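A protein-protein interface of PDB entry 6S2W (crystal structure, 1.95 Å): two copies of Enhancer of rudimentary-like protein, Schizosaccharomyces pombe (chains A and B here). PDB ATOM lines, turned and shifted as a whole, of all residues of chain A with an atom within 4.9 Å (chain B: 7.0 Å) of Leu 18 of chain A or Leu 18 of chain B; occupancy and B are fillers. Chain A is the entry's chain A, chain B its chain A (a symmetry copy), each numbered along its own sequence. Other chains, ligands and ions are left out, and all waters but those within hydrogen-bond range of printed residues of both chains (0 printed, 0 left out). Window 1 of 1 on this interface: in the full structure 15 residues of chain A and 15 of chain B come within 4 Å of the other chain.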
ATOM      1  N   ILE A  16     -15.998  -1.714  15.760  1.00  0.00           N
ATOM      2  CA  ILE A  16     -14.726  -1.483  16.412  1.00  0.00           C
ATOM      3  C   ILE A  16     -14.938  -2.100  17.800  1.00  0.00           C
ATOM      4  O   ILE A  16     -15.876  -1.707  18.508  1.00  0.00           O
ATOM      5  CB  ILE A  16     -14.257  -0.005  16.528  1.00  0.00           C
ATOM      6  CG1 ILE A  16     -14.015   0.631  15.155  1.00  0.00           C
ATOM      7  CG2 ILE A  16     -12.947   0.103  17.440  1.00  0.00           C
ATOM      8  CD1 ILE A  16     -13.895   2.136  15.280  1.00  0.00           C
ATOM      9  N   LEU A  17     -14.090  -3.059  18.176  1.00  0.00           N
ATOM     10  CA  LEU A  17     -14.158  -3.694  19.486  1.00  0.00           C
ATOM     11  C   LEU A  17     -13.092  -3.096  20.425  1.00  0.00           C
ATOM     12  O   LEU A  17     -11.926  -2.979  20.046  1.00  0.00           O
ATOM     13  CB  LEU A  17     -13.924  -5.203  19.317  1.00  0.00           C
ATOM     14  CG  LEU A  17     -14.910  -6.153  19.974  1.00  0.00           C
ATOM     15  CD1 LEU A  17     -16.367  -5.875  19.520  1.00  0.00           C
ATOM     16  CD2 LEU A  17     -14.545  -7.586  19.641  1.00  0.00           C
ATOM     17  N   LEU A  18     -13.483  -2.724  21.642  1.00  0.00           N
ATOM     18  CA  LEU A  18     -12.518  -2.168  22.617  1.00  0.00           C
ATOM     19  C   LEU A  18     -12.437  -3.153  23.746  1.00  0.00           C
ATOM     20  O   LEU A  18     -13.464  -3.475  24.332  1.00  0.00           O
ATOM     21  CB  LEU A  18     -12.958  -0.787  23.133  1.00  0.00           C
ATOM     22  CG  LEU A  18     -13.270   0.302  22.072  1.00  0.00           C
ATOM     23  CD1 LEU A  18     -13.769   1.551  22.771  1.00  0.00           C
ATOM     24  CD2 LEU A  18     -11.996   0.630  21.191  1.00  0.00           C
ATOM     25  N   ILE A  19     -11.255  -3.743  23.963  1.00  0.00           N
ATOM     26  CA  ILE A  19     -11.075  -4.704  25.041  1.00  0.00           C
ATOM     27  C   ILE A  19     -10.042  -4.184  26.046  1.00  0.00           C
ATOM     28  O   ILE A  19      -9.199  -3.339  25.731  1.00  0.00           O
ATOM     29  CB  ILE A  19     -10.788  -6.190  24.579  1.00  0.00           C
ATOM     30  CG1 ILE A  19      -9.319  -6.382  24.071  1.00  0.00           C
ATOM     31  CG2 ILE A  19     -11.838  -6.699  23.536  1.00  0.00           C
ATOM     32  CD1 ILE A  19      -8.868  -7.887  23.903  1.00  0.00           C
ATOM     33  N   GLN A  20     -10.085  -4.754  27.241  1.00  0.00           N
ATOM     34  CA  GLN A  20      -9.155  -4.476  28.332  1.00  0.00           C
ATOM     35  C   GLN A  20      -9.206  -5.623  29.331  1.00  0.00           C
ATOM     36  O   GLN A  20     -10.216  -6.332  29.444  1.00  0.00           O
ATOM     37  CB  GLN A  20      -9.467  -3.125  29.018  1.00  0.00           C
ATOM     38  CG  GLN A  20     -10.777  -3.101  29.793  1.00  0.00           C
ATOM     39  CD  GLN A  20     -10.996  -1.787  30.518  1.00  0.00           C
ATOM     40  OE1 GLN A  20     -10.657  -0.722  30.026  1.00  0.00           O
ATOM     41  NE2 GLN A  20     -11.581  -1.834  31.710  1.00  0.00           N
ATOM     42  N   ILE A  29      -6.712  -2.992  23.935  1.00  0.00           N
ATOM     43  CA  ILE A  29      -6.529  -3.382  22.541  1.00  0.00           C
ATOM     44  C   ILE A  29      -7.799  -3.192  21.764  1.00  0.00           C
ATOM     45  O   ILE A  29      -8.852  -3.633  22.206  1.00  0.00           O
ATOM     46  CB  ILE A  29      -5.978  -4.881  22.466  1.00  0.00           C
ATOM     47  CG1 ILE A  29      -4.590  -5.048  23.178  1.00  0.00           C
ATOM     48  CG2 ILE A  29      -5.946  -5.440  21.022  1.00  0.00           C
ATOM     49  CD1 ILE A  29      -3.397  -4.499  22.484  1.00  0.00           C
ATOM     50  N   TRP A  30      -7.697  -2.559  20.592  1.00  0.00           N
ATOM     51  CA  TRP A  30      -8.824  -2.397  19.721  1.00  0.00           C
ATOM     52  C   TRP A  30      -8.658  -3.251  18.497  1.00  0.00           C
ATOM     53  O   TRP A  30      -7.540  -3.564  18.108  1.00  0.00           O
ATOM     54  CB  TRP A  30      -9.115  -0.921  19.347  1.00  0.00           C
ATOM     55  CG  TRP A  30      -8.017  -0.294  18.538  1.00  0.00           C
ATOM     56  CD1 TRP A  30      -6.911   0.351  19.006  1.00  0.00           C
ATOM     57  CD2 TRP A  30      -7.967  -0.196  17.108  1.00  0.00           C
ATOM     58  NE1 TRP A  30      -6.155   0.813  17.953  1.00  0.00           N
ATOM     59  CE2 TRP A  30      -6.777   0.483  16.778  1.00  0.00           C
ATOM     60  CE3 TRP A  30      -8.779  -0.698  16.066  1.00  0.00           C
ATOM     61  CZ2 TRP A  30      -6.381   0.699  15.449  1.00  0.00           C
ATOM     62  CZ3 TRP A  30      -8.406  -0.441  14.748  1.00  0.00           C
ATOM     63  CH2 TRP A  30      -7.226   0.264  14.455  1.00  0.00           C
ATOM     64  N   ASP A  73     -12.957  -6.980  29.990  1.00  0.00           N
ATOM     65  CA  ASP A  73     -14.084  -6.106  29.760  1.00  0.00           C
ATOM     66  C   ASP A  73     -14.016  -5.776  28.288  1.00  0.00           C
ATOM     67  O   ASP A  73     -12.918  -5.699  27.717  1.00  0.00           O
ATOM     68  CB  ASP A  73     -14.028  -4.835  30.627  1.00  0.00           C
ATOM     69  CG  ASP A  73     -15.389  -4.240  30.941  1.00  0.00           C
ATOM     70  OD1 ASP A  73     -16.357  -4.542  30.207  1.00  0.00           O
ATOM     71  OD2 ASP A  73     -15.482  -3.441  31.897  1.00  0.00           O
ATOM     72  N   CYS A  74     -15.182  -5.613  27.658  1.00  0.00           N
ATOM     73  CA  CYS A  74     -15.278  -5.340  26.227  1.00  0.00           C
ATOM     74  C   CYS A  74     -16.451  -4.413  25.892  1.00  0.00           C
ATOM     75  O   CYS A  74     -17.503  -4.505  26.521  1.00  0.00           O
ATOM     76  CB  CYS A  74     -15.361  -6.653  25.452  1.00  0.00           C
ATOM     77  SG  CYS A  74     -15.477  -6.457  23.657  1.00  0.00           S
ATOM     78  N   VAL A  75     -16.273  -3.534  24.897  1.00  0.00           N
ATOM     79  CA  VAL A  75     -17.328  -2.629  24.440  1.00  0.00           C
ATOM     80  C   VAL A  75     -17.302  -2.585  22.932  1.00  0.00           C
ATOM     81  O   VAL A  75     -16.270  -2.239  22.358  1.00  0.00           O
ATOM     82  CB  VAL A  75     -17.291  -1.197  25.095  1.00  0.00           C
ATOM     83  CG1 VAL A  75     -18.005  -0.142  24.234  1.00  0.00           C
ATOM     84  CG2 VAL A  75     -17.914  -1.220  26.482  1.00  0.00           C
ATOM     85  N   LEU A  77     -18.395  -0.831  19.344  1.00  0.00           N
ATOM     86  CA  LEU A  77     -18.780   0.435  18.724  1.00  0.00           C
ATOM     87  C   LEU A  77     -19.277   0.018  17.346  1.00  0.00           C
ATOM     88  O   LEU A  77     -18.506  -0.557  16.572  1.00  0.00           O
ATOM     89  CB  LEU A  77     -17.583   1.402  18.611  1.00  0.00           C
ATOM     90  CG  LEU A  77     -16.851   1.805  19.936  1.00  0.00           C
ATOM     91  CD1 LEU A  77     -15.666   2.694  19.651  1.00  0.00           C
ATOM     92  CD2 LEU A  77     -17.744   2.546  20.861  1.00  0.00           C
ATOM     93  N   ILE B  15     -13.175  11.798  24.080  1.00  0.00           N
ATOM     94  CA  ILE B  15     -12.419  11.279  22.939  1.00  0.00           C
ATOM     95  C   ILE B  15     -11.928   9.859  23.188  1.00  0.00           C
ATOM     96  O   ILE B  15     -11.427   9.543  24.265  1.00  0.00           O
ATOM     97  CB  ILE B  15     -11.272  12.244  22.492  1.00  0.00           C
ATOM     98  CG1 ILE B  15     -11.838  13.567  21.929  1.00  0.00           C
ATOM     99  CG2 ILE B  15     -10.311  11.590  21.466  1.00  0.00           C
ATOM    100  CD1 ILE B  15     -10.826  14.678  21.715  1.00  0.00           C
ATOM    101  N   ILE B  16     -12.054   9.010  22.172  1.00  0.00           N
ATOM    102  CA  ILE B  16     -11.454   7.692  22.187  1.00  0.00           C
ATOM    103  C   ILE B  16     -10.368   7.801  21.110  1.00  0.00           C
ATOM    104  O   ILE B  16     -10.679   8.134  19.958  1.00  0.00           O
ATOM    105  CB  ILE B  16     -12.399   6.490  21.902  1.00  0.00           C
ATOM    106  CG1 ILE B  16     -13.483   6.342  22.974  1.00  0.00           C
ATOM    107  CG2 ILE B  16     -11.561   5.135  21.754  1.00  0.00           C
ATOM    108  CD1 ILE B  16     -14.571   5.401  22.505  1.00  0.00           C
ATOM    109  N   LEU B  17      -9.113   7.539  21.483  1.00  0.00           N
ATOM    110  CA  LEU B  17      -7.997   7.566  20.546  1.00  0.00           C
ATOM    111  C   LEU B  17      -7.625   6.133  20.119  1.00  0.00           C
ATOM    112  O   LEU B  17      -7.474   5.252  20.966  1.00  0.00           O
ATOM    113  CB  LEU B  17      -6.796   8.242  21.225  1.00  0.00           C
ATOM    114  CG  LEU B  17      -6.085   9.351  20.471  1.00  0.00           C
ATOM    115  CD1 LEU B  17      -7.059  10.485  20.059  1.00  0.00           C
ATOM    116  CD2 LEU B  17      -4.976   9.929  21.328  1.00  0.00           C
ATOM    117  N   LEU B  18      -7.471   5.899  18.818  1.00  0.00           N
ATOM    118  CA  LEU B  18      -7.084   4.558  18.324  1.00  0.00           C
ATOM    119  C   LEU B  18      -5.724   4.706  17.708  1.00  0.00           C
ATOM    120  O   LEU B  18      -5.560   5.529  16.815  1.00  0.00           O
ATOM    121  CB  LEU B  18      -8.090   4.016  17.293  1.00  0.00           C
ATOM    122  CG  LEU B  18      -9.584   3.976  17.711  1.00  0.00           C
ATOM    123  CD1 LEU B  18     -10.417   3.501  16.537  1.00  0.00           C
ATOM    124  CD2 LEU B  18      -9.806   3.037  18.966  1.00  0.00           C
ATOM    125  N   ILE B  19      -4.718   4.025  18.270  1.00  0.00           N
ATOM    126  CA  ILE B  19      -3.365   4.096  17.738  1.00  0.00           C
ATOM    127  C   ILE B  19      -2.910   2.713  17.262  1.00  0.00           C
ATOM    128  O   ILE B  19      -3.425   1.677  17.694  1.00  0.00           O
ATOM    129  CB  ILE B  19      -2.305   4.800  18.679  1.00  0.00           C
ATOM    130  CG1 ILE B  19      -1.863   3.882  19.867  1.00  0.00           C
ATOM    131  CG2 ILE B  19      -2.794   6.202  19.174  1.00  0.00           C
ATOM    132  CD1 ILE B  19      -0.585   4.384  20.651  1.00  0.00           C
ATOM    133  N   GLN B  20      -1.892   2.716  16.414  1.00  0.00           N
ATOM    134  CA  GLN B  20      -1.242   1.521  15.886  1.00  0.00           C
ATOM    135  C   GLN B  20       0.135   1.897  15.359  1.00  0.00           C
ATOM    136  O   GLN B  20       0.383   3.050  14.975  1.00  0.00           O
ATOM    137  CB  GLN B  20      -2.094   0.845  14.786  1.00  0.00           C
ATOM    138  CG  GLN B  20      -2.216   1.654  13.501  1.00  0.00           C
ATOM    139  CD  GLN B  20      -2.986   0.914  12.424  1.00  0.00           C
ATOM    140  OE1 GLN B  20      -3.946   0.209  12.695  1.00  0.00           O
ATOM    141  NE2 GLN B  20      -2.583   1.066  11.167  1.00  0.00           N
ATOM    142  N   THR B  27      -0.114  -3.754  18.497  1.00  0.00           N
ATOM    143  CA  THR B  27       0.171  -2.319  18.723  1.00  0.00           C
ATOM    144  C   THR B  27      -1.128  -1.488  18.681  1.00  0.00           C
ATOM    145  O   THR B  27      -1.071  -0.263  18.838  1.00  0.00           O
ATOM    146  CB  THR B  27       1.184  -1.762  17.696  1.00  0.00           C
ATOM    147  OG1 THR B  27       0.548  -1.690  16.409  1.00  0.00           O
ATOM    148  CG2 THR B  27       2.517  -2.560  17.646  1.00  0.00           C
ATOM    149  N   ARG B  28      -2.281  -2.139  18.444  1.00  0.00           N
ATOM    150  CA  ARG B  28      -3.561  -1.441  18.371  1.00  0.00           C
ATOM    151  C   ARG B  28      -4.093  -1.115  19.788  1.00  0.00           C
ATOM    152  O   ARG B  28      -4.857  -1.864  20.394  1.00  0.00           O
ATOM    153  CB  ARG B  28      -4.574  -2.189  17.474  1.00  0.00           C
ATOM    154  CG  ARG B  28      -4.119  -2.187  16.020  1.00  0.00           C
ATOM    155  CD  ARG B  28      -5.111  -2.814  15.060  1.00  0.00           C
ATOM    156  NE  ARG B  28      -5.020  -2.173  13.741  1.00  0.00           N
ATOM    157  CZ  ARG B  28      -5.863  -2.365  12.730  1.00  0.00           C
ATOM    158  NH1 ARG B  28      -5.707  -1.693  11.595  1.00  0.00           N
ATOM    159  NH2 ARG B  28      -6.873  -3.222  12.847  1.00  0.00           N
ATOM    160  N   ILE B  29      -3.663   0.024  20.290  1.00  0.00           N
ATOM    161  CA  ILE B  29      -3.965   0.483  21.642  1.00  0.00           C
ATOM    162  C   ILE B  29      -4.959   1.607  21.613  1.00  0.00           C
ATOM    163  O   ILE B  29      -4.779   2.556  20.861  1.00  0.00           O
ATOM    164  CB  ILE B  29      -2.610   0.875  22.396  1.00  0.00           C
ATOM    165  CG1 ILE B  29      -1.624  -0.337  22.530  1.00  0.00           C
ATOM    166  CG2 ILE B  29      -2.858   1.559  23.763  1.00  0.00           C
ATOM    167  CD1 ILE B  29      -1.960  -1.383  23.529  1.00  0.00           C
ATOM    168  N   TRP B  30      -5.994   1.516  22.454  1.00  0.00           N
ATOM    169  CA  TRP B  30      -6.958   2.569  22.580  1.00  0.00           C
ATOM    170  C   TRP B  30      -6.815   3.243  23.914  1.00  0.00           C
ATOM    171  O   TRP B  30      -6.347   2.635  24.868  1.00  0.00           O
ATOM    172  CB  TRP B  30      -8.418   2.109  22.330  1.00  0.00           C
ATOM    173  CG  TRP B  30      -8.906   1.128  23.357  1.00  0.00           C
ATOM    174  CD1 TRP B  30      -8.786  -0.229  23.325  1.00  0.00           C
ATOM    175  CD2 TRP B  30      -9.662   1.440  24.535  1.00  0.00           C
ATOM    176  NE1 TRP B  30      -9.387  -0.780  24.433  1.00  0.00           N
ATOM    177  CE2 TRP B  30      -9.926   0.223  25.195  1.00  0.00           C
ATOM    178  CE3 TRP B  30     -10.068   2.649  25.143  1.00  0.00           C
ATOM    179  CZ2 TRP B  30     -10.598   0.168  26.426  1.00  0.00           C
ATOM    180  CZ3 TRP B  30     -10.776   2.586  26.342  1.00  0.00           C
ATOM    181  CH2 TRP B  30     -11.046   1.353  26.960  1.00  0.00           C
ATOM    182  N   SER B  31      -7.219   4.508  23.972  1.00  0.00           N
ATOM    183  CA  SER B  31      -7.187   5.301  25.199  1.00  0.00           C
ATOM    184  C   SER B  31      -8.382   6.248  25.237  1.00  0.00           C
ATOM    185  O   SER B  31      -8.887   6.683  24.182  1.00  0.00           O
ATOM    186  CB  SER B  31      -5.871   6.072  25.305  1.00  0.00           C
ATOM    187  OG  SER B  31      -5.624   6.783  24.097  1.00  0.00           O
ATOM    188  N   ASP B  73       0.159   5.419  13.373  1.00  0.00           N
ATOM    189  CA  ASP B  73      -1.059   5.906  12.768  1.00  0.00           C
ATOM    190  C   ASP B  73      -2.012   6.091  13.925  1.00  0.00           C
ATOM    191  O   ASP B  73      -1.949   5.339  14.910  1.00  0.00           O
ATOM    192  CB  ASP B  73      -1.626   4.931  11.719  1.00  0.00           C
ATOM    193  CG  ASP B  73      -2.443   5.602  10.630  1.00  0.00           C
ATOM    194  OD1 ASP B  73      -2.915   6.739  10.851  1.00  0.00           O
ATOM    195  OD2 ASP B  73      -2.646   4.975   9.568  1.00  0.00           O
ATOM    196  N   CYS B  74      -2.875   7.105  13.833  1.00  0.00           N
ATOM    197  CA  CYS B  74      -3.823   7.439  14.892  1.00  0.00           C
ATOM    198  C   CYS B  74      -5.150   7.963  14.337  1.00  0.00           C
ATOM    199  O   CYS B  74      -5.157   8.670  13.331  1.00  0.00           O
ATOM    200  CB  CYS B  74      -3.188   8.432  15.863  1.00  0.00           C
ATOM    201  SG  CYS B  74      -4.260   8.924  17.236  1.00  0.00           S
ATOM    202  N   VAL B  75      -6.267   7.630  14.998  1.00  0.00           N
ATOM    203  CA  VAL B  75      -7.594   8.107  14.607  1.00  0.00           C
ATOM    204  C   VAL B  75      -8.352   8.489  15.854  1.00  0.00           C
ATOM    205  O   VAL B  75      -8.528   7.645  16.733  1.00  0.00           O
ATOM    206  CB  VAL B  75      -8.398   7.120  13.679  1.00  0.00           C
ATOM    207  CG1 VAL B  75      -9.914   7.361  13.746  1.00  0.00           C
ATOM    208  CG2 VAL B  75      -7.932   7.235  12.235  1.00  0.00           C
ATOM    209  N   PRO B  76      -8.816   9.758  15.949  1.00  0.00           N
ATOM    210  CA  PRO B  76      -9.670  10.138  17.084  1.00  0.00           C
ATOM    211  C   PRO B  76     -11.166   9.890  16.783  1.00  0.00           C
ATOM    212  O   PRO B  76     -11.662  10.147  15.671  1.00  0.00           O
ATOM    213  CB  PRO B  76      -9.394  11.643  17.238  1.00  0.00           C
ATOM    214  CG  PRO B  76      -8.822  12.098  15.873  1.00  0.00           C
ATOM    215  CD  PRO B  76      -8.637  10.886  15.008  1.00  0.00           C
ATOM    216  N   LEU B  77     -11.889   9.423  17.793  1.00  0.00           N
ATOM    217  CA  LEU B  77     -13.336   9.221  17.762  1.00  0.00           C
ATOM    218  C   LEU B  77     -13.857  10.229  18.777  1.00  0.00           C
ATOM    219  O   LEU B  77     -13.496  10.146  19.954  1.00  0.00           O
ATOM    220  CB  LEU B  77     -13.720   7.781  18.164  1.00  0.00           C
ATOM    221  CG  LEU B  77     -13.127   6.610  17.310  1.00  0.00           C
ATOM    222  CD1 LEU B  77     -13.537   5.271  17.872  1.00  0.00           C
ATOM    223  CD2 LEU B  77     -13.592   6.657  15.903  1.00  0.00           C
ATOM    224  N   TYR B  86     -20.215   8.489  18.535  1.00  0.00           N
ATOM    225  CA  TYR B  86     -18.812   8.763  18.287  1.00  0.00           C
ATOM    226  C   TYR B  86     -18.595   9.062  16.822  1.00  0.00           C
ATOM    227  O   TYR B  86     -18.904   8.252  15.949  1.00  0.00           O
ATOM    228  CB  TYR B  86     -17.938   7.580  18.705  1.00  0.00           C
ATOM    229  CG  TYR B  86     -17.620   7.555  20.177  1.00  0.00           C
ATOM    230  CD1 TYR B  86     -16.703   8.450  20.729  1.00  0.00           C
ATOM    231  CD2 TYR B  86     -18.298   6.695  21.039  1.00  0.00           C
ATOM    232  CE1 TYR B  86     -16.427   8.451  22.094  1.00  0.00           C
ATOM    233  CE2 TYR B  86     -18.028   6.687  22.409  1.00  0.00           C
ATOM    234  CZ  TYR B  86     -17.117   7.593  22.933  1.00  0.00           C
ATOM    235  OH  TYR B  86     -16.849   7.583  24.276  1.00  0.00           O
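Leu 18 of chain A touches its own counterpart, Leu 18 of chain B.
Gln 20 of chain A touches Trp 30 of chain B, and with the chains exchanged Trp 30 of chain A touches Gln 20 of chain B.
Ile 29 of chain A touches Trp 30 of chain B, and with the chains exchanged Trp 30 of chain A touches Ile 29 of chain B.
Trp 30 of chain B touches its own counterpart, Trp 30 of chain A.
Positions printed for both chains: 16, 17, 18, 19, 20, 29, 30, 73, 74, 75 and 77.
Of the 16 pairs that touch across the chains among the printed residues, 14 have their exchanged pair printed and touching as well.
O of Leu 18 of chain B lies within hydrogen-bond range of N of Val 75 of chain B, at 2.9 Å.
The side-chain sulfur of Cys 74 of chain A lies close to the backbone carbonyl oxygen of Leu 18 of chain A, at 3.7 Å.
The backbone carbonyl oxygen (O) of Leu 18 of chain B lies close to the side-chain sulfur (SG) of Cys 74 of chain B, at 3.7 Å.
OE1 of Gln 20 of chain B is in hydrogen-bond range of NE of Arg 28 of chain B (2.8 Å).
N of Ile 19 of chain A lies within hydrogen-bond range of O of Ile 29 of chain A (3.0 Å).
O of Ile 29 of chain B sits at hydrogen-bond distance from N of Ile 19 of chain B, 3.0 Å away.
Leu 18 of chain B touches Ile 16 of chain A (CD1 to CD1, 3.9 Å).
Leu 18 of chain A touches Ile 16 of chain B.
Leu 18 of chain A touches Leu 18 of chain B (CD2 to CD2, 3.9 Å).
CB of Leu 18 of chain A touches NE1 of Trp 30 of chain B, at 3.8 Å.
CD1 of Ile 29 of chain B touches CD1 of Ile 29 of chain A (3.6 Å).
Ile 29 of chain A touches Trp 30 of chain B (C to CD1, 3.5 Å).
Trp 30 of chain A touches Leu 18 of chain B.
Trp 30 of chain A touches Gln 20 of chain B (CZ2 to OE1, 3.7 Å).
Trp 30 of chain A touches Trp 30 of chain B (N to CD1, 3.8 Å).
Leu 77 of chain A touches Leu 77 of chain B (CD1 to CD1, 3.8 Å).
Leu 18 of chain A touches just these residues of chain B: Ile 16, Leu 18 and Trp 30.
Leu 18 of chain B touches three residues of chain A.
Of the printed residues of chain B, Trp 30 of chain A touches Leu 18, Ile 19, Gln 20, Arg 28, Ile 29 and Trp 30.
Printed residues of chain B within 4 Å of Gln 20 of chain A: Trp 30.
Of the printed residues of chain B, Ile 29 of chain A touches Arg 28 (3.1 Å), Ile 29 (3.6 Å) and Trp 30 (3.5 Å).
The nearest residue of chain B that does not touch Leu 18 of chain A is Leu 77 of chain B (5.9 Å).
The nearest printed residue of chain A that does not touch Leu 18 of chain B is Leu 77 of chain A (5.9 Å).
The nearest printed residue of chain B that does not touch Leu 77 of chain A is Ile 16 of chain B (4.1 Å).
Of the 17 printed residues of chain B, 8 touch a printed residue of chain A.
Printed residues of chain B that touch a printed residue of chain A: Ile 16, Leu 18, Ile 19, Gln 20, Arg 28, Ile 29, Trp 30 and Leu 77.
Hydrophobic or aromatic side chains of chain B that line the printed part of chain A: Ile 16, Leu 18, Ile 29, Trp 30 and Leu 77.
Printed residues of chain A that touch a printed residue of chain B: Ile 16, Leu 18, Ile 19, Gln 20, Ile 29, Trp 30 and Leu 77.
Among the printed residues, 16 pairs touch across the chains.
Among the printed residues, no Asp or Glu carboxylate lies within 4 Å of a Lys or Arg side-chain nitrogen of the other chain.
The backbone carbonyl oxygen (O) of Ile 19 of chain A sits at hydrogen-bond distance from the indole nitrogen (NE1) of Trp 30 of chain B, at 2.9 Å.
NE1 of Trp 30 of chain A lies within hydrogen-bond range of O of Ile 19 of chain B.
The backbone NH (N) of Trp 30 of chain A sits at hydrogen-bond distance from the backbone carbonyl oxygen (O) of Arg 28 of chain B.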
